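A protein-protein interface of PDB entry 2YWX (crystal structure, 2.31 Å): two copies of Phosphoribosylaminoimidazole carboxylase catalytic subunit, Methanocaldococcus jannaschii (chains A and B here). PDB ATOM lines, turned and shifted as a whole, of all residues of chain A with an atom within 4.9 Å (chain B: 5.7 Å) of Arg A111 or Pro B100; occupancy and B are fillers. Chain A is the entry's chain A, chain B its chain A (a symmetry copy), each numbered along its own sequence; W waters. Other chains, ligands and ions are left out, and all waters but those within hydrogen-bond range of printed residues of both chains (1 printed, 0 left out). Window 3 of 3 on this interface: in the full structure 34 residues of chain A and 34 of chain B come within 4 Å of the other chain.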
ATOM      1  N   LYS A  17      25.785 -18.999  28.866  1.00  0.00           N
ATOM      2  CA  LYS A  17      25.108 -20.194  29.330  1.00  0.00           C
ATOM      3  C   LYS A  17      26.080 -20.901  30.266  1.00  0.00           C
ATOM      4  O   LYS A  17      25.695 -21.404  31.321  1.00  0.00           O
ATOM      5  CB  LYS A  17      24.768 -21.106  28.157  1.00  0.00           C
ATOM      6  CG  LYS A  17      23.702 -20.560  27.232  1.00  0.00           C
ATOM      7  CD  LYS A  17      23.401 -21.568  26.127  1.00  0.00           C
ATOM      8  CE  LYS A  17      22.420 -21.029  25.101  1.00  0.00           C
ATOM      9  NZ  LYS A  17      22.076 -22.087  24.102  1.00  0.00           N
ATOM     10  N   VAL A  80      32.920 -25.983  22.249  1.00  0.00           N
ATOM     11  CA  VAL A  80      31.491 -25.764  22.082  1.00  0.00           C
ATOM     12  C   VAL A  80      31.296 -25.229  20.678  1.00  0.00           C
ATOM     13  O   VAL A  80      31.632 -24.083  20.398  1.00  0.00           O
ATOM     14  CB  VAL A  80      30.934 -24.728  23.087  1.00  0.00           C
ATOM     15  CG1 VAL A  80      29.435 -24.529  22.846  1.00  0.00           C
ATOM     16  CG2 VAL A  80      31.177 -25.200  24.512  1.00  0.00           C
ATOM     17  N   VAL A 107      31.169 -31.097  22.943  1.00  0.00           N
ATOM     18  CA  VAL A 107      29.794 -31.221  23.407  1.00  0.00           C
ATOM     19  C   VAL A 107      28.928 -30.706  22.271  1.00  0.00           C
ATOM     20  O   VAL A 107      29.453 -30.188  21.284  1.00  0.00           O
ATOM     21  CB  VAL A 107      29.512 -30.402  24.699  1.00  0.00           C
ATOM     22  CG1 VAL A 107      30.299 -30.974  25.858  1.00  0.00           C
ATOM     23  CG2 VAL A 107      29.856 -28.945  24.494  1.00  0.00           C
ATOM     24  N   GLY A 108      27.612 -30.855  22.409  1.00  0.00           N
ATOM     25  CA  GLY A 108      26.686 -30.420  21.376  1.00  0.00           C
ATOM     26  C   GLY A 108      26.797 -28.966  20.966  1.00  0.00           C
ATOM     27  O   GLY A 108      27.401 -28.154  21.664  1.00  0.00           O
ATOM     28  N   ILE A 109      26.205 -28.639  19.822  1.00  0.00           N
ATOM     29  CA  ILE A 109      26.236 -27.283  19.293  1.00  0.00           C
ATOM     30  C   ILE A 109      25.453 -26.327  20.202  1.00  0.00           C
ATOM     31  O   ILE A 109      24.300 -26.593  20.566  1.00  0.00           O
ATOM     32  CB  ILE A 109      25.658 -27.253  17.857  1.00  0.00           C
ATOM     33  CG1 ILE A 109      26.381 -28.292  16.994  1.00  0.00           C
ATOM     34  CG2 ILE A 109      25.862 -25.882  17.233  1.00  0.00           C
ATOM     35  CD1 ILE A 109      25.823 -28.446  15.593  1.00  0.00           C
ATOM     36  N   ASP A 110      26.107 -25.220  20.566  1.00  0.00           N
ATOM     37  CA  ASP A 110      25.543 -24.186  21.437  1.00  0.00           C
ATOM     38  C   ASP A 110      25.304 -24.657  22.858  1.00  0.00           C
ATOM     39  O   ASP A 110      24.613 -23.993  23.626  1.00  0.00           O
ATOM     40  CB  ASP A 110      24.221 -23.651  20.880  1.00  0.00           C
ATOM     41  CG  ASP A 110      24.382 -22.993  19.534  1.00  0.00           C
ATOM     42  OD1 ASP A 110      25.520 -22.614  19.193  1.00  0.00           O
ATOM     43  OD2 ASP A 110      23.368 -22.840  18.821  1.00  0.00           O
ATOM     44  N   ARG A 111      25.880 -25.796  23.212  1.00  0.00           N
ATOM     45  CA  ARG A 111      25.702 -26.348  24.539  1.00  0.00           C
ATOM     46  C   ARG A 111      26.709 -25.823  25.571  1.00  0.00           C
ATOM     47  O   ARG A 111      27.499 -26.581  26.141  1.00  0.00           O
ATOM     48  CB  ARG A 111      25.750 -27.879  24.440  1.00  0.00           C
ATOM     49  CG  ARG A 111      24.561 -28.463  23.686  1.00  0.00           C
ATOM     50  CD  ARG A 111      23.365 -28.662  24.618  1.00  0.00           C
ATOM     51  NE  ARG A 111      22.081 -28.569  23.932  1.00  0.00           N
ATOM     52  CZ  ARG A 111      21.493 -27.422  23.589  1.00  0.00           C
ATOM     53  NH1 ARG A 111      22.075 -26.264  23.869  1.00  0.00           N
ATOM     54  NH2 ARG A 111      20.318 -27.424  22.966  1.00  0.00           N
ATOM     55  N   GLY A 112      26.661 -24.520  25.824  1.00  0.00           N
ATOM     56  CA  GLY A 112      27.566 -23.914  26.787  1.00  0.00           C
ATOM     57  C   GLY A 112      27.337 -24.434  28.193  1.00  0.00           C
ATOM     58  O   GLY A 112      28.269 -24.568  28.987  1.00  0.00           O
ATOM     59  N   GLU A 113      26.081 -24.730  28.500  1.00  0.00           N
ATOM     60  CA  GLU A 113      25.717 -25.251  29.807  1.00  0.00           C
ATOM     61  C   GLU A 113      26.344 -26.631  30.014  1.00  0.00           C
ATOM     62  O   GLU A 113      26.904 -26.916  31.076  1.00  0.00           O
ATOM     63  CB  GLU A 113      24.192 -25.324  29.917  1.00  0.00           C
ATOM     64  CG  GLU A 113      23.676 -25.710  31.278  1.00  0.00           C
ATOM     65  CD  GLU A 113      22.181 -25.446  31.426  1.00  0.00           C
ATOM     66  OE1 GLU A 113      21.782 -24.257  31.405  1.00  0.00           O
ATOM     67  OE2 GLU A 113      21.407 -26.429  31.560  1.00  0.00           O
ATOM     68  N   ASN A 114      26.268 -27.482  28.996  1.00  0.00           N
ATOM     69  CA  ASN A 114      26.854 -28.821  29.102  1.00  0.00           C
ATOM     70  C   ASN A 114      28.372 -28.753  29.157  1.00  0.00           C
ATOM     71  O   ASN A 114      29.017 -29.635  29.717  1.00  0.00           O
ATOM     72  CB  ASN A 114      26.410 -29.716  27.941  1.00  0.00           C
ATOM     73  CG  ASN A 114      25.192 -30.547  28.288  1.00  0.00           C
ATOM     74  OD1 ASN A 114      24.739 -31.379  27.500  1.00  0.00           O
ATOM     75  ND2 ASN A 114      24.655 -30.325  29.482  1.00  0.00           N
ATOM     76  N   ALA A 115      28.937 -27.696  28.580  1.00  0.00           N
ATOM     77  CA  ALA A 115      30.384 -27.510  28.620  1.00  0.00           C
ATOM     78  C   ALA A 115      30.817 -27.187  30.056  1.00  0.00           C
ATOM     79  O   ALA A 115      31.828 -27.697  30.531  1.00  0.00           O
ATOM     80  CB  ALA A 115      30.801 -26.394  27.674  1.00  0.00           C
ATOM     81  N   MET A 141      17.296 -31.533  38.777  1.00  0.00           N
ATOM     82  CA  MET A 141      16.804 -31.800  37.427  1.00  0.00           C
ATOM     83  C   MET A 141      15.704 -32.842  37.362  1.00  0.00           C
ATOM     84  O   MET A 141      14.777 -32.707  36.573  1.00  0.00           O
ATOM     85  CB  MET A 141      17.943 -32.236  36.505  1.00  0.00           C
ATOM     86  CG  MET A 141      18.882 -31.130  36.072  1.00  0.00           C
ATOM     87  SD  MET A 141      20.017 -31.724  34.775  1.00  0.00           S
ATOM     88  CE  MET A 141      19.458 -30.735  33.394  1.00  0.00           C
ATOM     89  N   GLN B  97      25.151 -34.928  20.725  1.00  0.00           N
ATOM     90  CA  GLN B  97      23.983 -34.089  20.958  1.00  0.00           C
ATOM     91  C   GLN B  97      23.204 -34.408  22.233  1.00  0.00           C
ATOM     92  O   GLN B  97      21.979 -34.521  22.202  1.00  0.00           O
ATOM     93  CB  GLN B  97      23.040 -34.169  19.755  1.00  0.00           C
ATOM     94  CG  GLN B  97      23.507 -33.379  18.542  1.00  0.00           C
ATOM     95  CD  GLN B  97      23.572 -31.885  18.815  1.00  0.00           C
ATOM     96  OE1 GLN B  97      24.424 -31.414  19.572  1.00  0.00           O
ATOM     97  NE2 GLN B  97      22.661 -31.133  18.208  1.00  0.00           N
ATOM     98  N   MET B  98      23.906 -34.550  23.352  1.00  0.00           N
ATOM     99  CA  MET B  98      23.242 -34.832  24.619  1.00  0.00           C
ATOM    100  C   MET B  98      22.437 -33.612  25.025  1.00  0.00           C
ATOM    101  O   MET B  98      22.676 -32.511  24.529  1.00  0.00           O
ATOM    102  CB  MET B  98      24.267 -35.165  25.706  1.00  0.00           C
ATOM    103  CG  MET B  98      24.792 -36.591  25.641  1.00  0.00           C
ATOM    104  SD  MET B  98      23.495 -37.832  25.921  1.00  0.00           S
ATOM    105  CE  MET B  98      23.502 -37.955  27.708  1.00  0.00           C
ATOM    106  N   PRO B  99      21.460 -33.791  25.924  1.00  0.00           N
ATOM    107  CA  PRO B  99      20.616 -32.688  26.391  1.00  0.00           C
ATOM    108  C   PRO B  99      21.228 -31.999  27.615  1.00  0.00           C
ATOM    109  O   PRO B  99      21.994 -32.606  28.366  1.00  0.00           O
ATOM    110  CB  PRO B  99      19.310 -33.395  26.715  1.00  0.00           C
ATOM    111  CG  PRO B  99      19.815 -34.654  27.360  1.00  0.00           C
ATOM    112  CD  PRO B  99      20.964 -35.079  26.443  1.00  0.00           C
ATOM    113  N   PRO B 100      20.886 -30.718  27.834  1.00  0.00           N
ATOM    114  CA  PRO B 100      21.406 -29.949  28.969  1.00  0.00           C
ATOM    115  C   PRO B 100      21.366 -30.689  30.305  1.00  0.00           C
ATOM    116  O   PRO B 100      20.363 -31.314  30.645  1.00  0.00           O
ATOM    117  CB  PRO B 100      20.529 -28.703  28.957  1.00  0.00           C
ATOM    118  CG  PRO B 100      20.302 -28.486  27.495  1.00  0.00           C
ATOM    119  CD  PRO B 100      19.979 -29.888  27.018  1.00  0.00           C
ATOM    120  N   GLY B 101      22.469 -30.618  31.050  1.00  0.00           N
ATOM    121  CA  GLY B 101      22.548 -31.269  32.349  1.00  0.00           C
ATOM    122  C   GLY B 101      23.332 -32.569  32.405  1.00  0.00           C
ATOM    123  O   GLY B 101      23.976 -32.862  33.422  1.00  0.00           O
ATOM    124  N   ILE B 102      23.274 -33.358  31.330  1.00  0.00           N
ATOM    125  CA  ILE B 102      23.978 -34.642  31.272  1.00  0.00           C
ATOM    126  C   ILE B 102      24.943 -34.651  30.081  1.00  0.00           C
ATOM    127  O   ILE B 102      24.659 -35.233  29.039  1.00  0.00           O
ATOM    128  CB  ILE B 102      22.980 -35.833  31.114  1.00  0.00           C
ATOM    129  CG1 ILE B 102      21.835 -35.719  32.138  1.00  0.00           C
ATOM    130  CG2 ILE B 102      23.723 -37.164  31.264  1.00  0.00           C
ATOM    131  CD1 ILE B 102      22.256 -35.847  33.592  1.00  0.00           C
HETATM  132  O   HOH W   1      25.984 -31.581  24.863  1.00  0.00           O
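Among the printed residues, merely in contact across the chains: Met A141 with Pro B100 (3.0 Å), Gly A108 with Gln B97 (3.1 Å), Met A141 with Gly B101 (3.3 Å), Asn A114 with Pro B100 (3.3 Å), Glu A113 with Pro B100 (3.6 Å), Asn A114 with Met B98 (3.8 Å), Asn A114 with Ile B102 (3.8 Å), Arg A111 with Met B98 (3.9 Å) and Arg A111 with Pro B100 (3.96 Å).
The side-chain amide oxygen of Gln B97 sits at hydrogen-bond distance from the backbone NH of Ile A109, at 3.3 Å. The side-chain amide oxygen (OD1) of Asn A114 lies close to the backbone carbonyl oxygen (O) of Pro B99, 3.1 Å away. ND2 of Asn A114 sits close to N of Gly B101 (2.7 Å).
Of the printed residues of chain B, Arg A111 touches Met B98 (3.9 Å) and Pro B100 (3.96 Å). Of the printed residues of chain A, Pro B100 touches Arg A111 (3.96 Å), Glu A113 (3.6 Å), Asn A114 (3.3 Å) and Met A141 (3.0 Å). Of the printed residues of chain A, Gln B97 touches Gly A108 (3.1 Å) and Ile A109 (3.3 Å). Of the printed residues of chain A, Pro B99 touches Asn A114. Printed residues of chain B within 4 Å of Gly A108: Gln B97. Of the printed residues of chain A, Gly B101 touches Asn A114 and Met A141. Of the printed residues of chain B, Glu A113 touches Pro B100. The nearest printed residue of chain A that does not touch Met B98 is Gly A108 (5.3 Å).
Of the 12 printed residues of chain A, 6 touch a printed residue of chain B. Of the 6 printed residues of chain B, 6 touch a printed residue of chain A. Hydrophobic or aromatic side chains of chain B within 4 Å of the printed part of chain A: Pro B100. Among the printed residues, no Asp or Glu carboxylate lies within 4 Å of a Lys or Arg side-chain nitrogen of the other chain.
Water W1 lies within hydrogen-bond range of the side-chain amide oxygen (OD1) of Asn A114 (2.9 Å), the backbone NH (N) of Gly A108 (3.0 Å) and the backbone carbonyl oxygen (O) of Met B98 (3.5 Å).
No position is printed for both chains. Of the 12 pairs that touch across the chains among the printed residues, none has its exchanged pair printed and touching as well.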
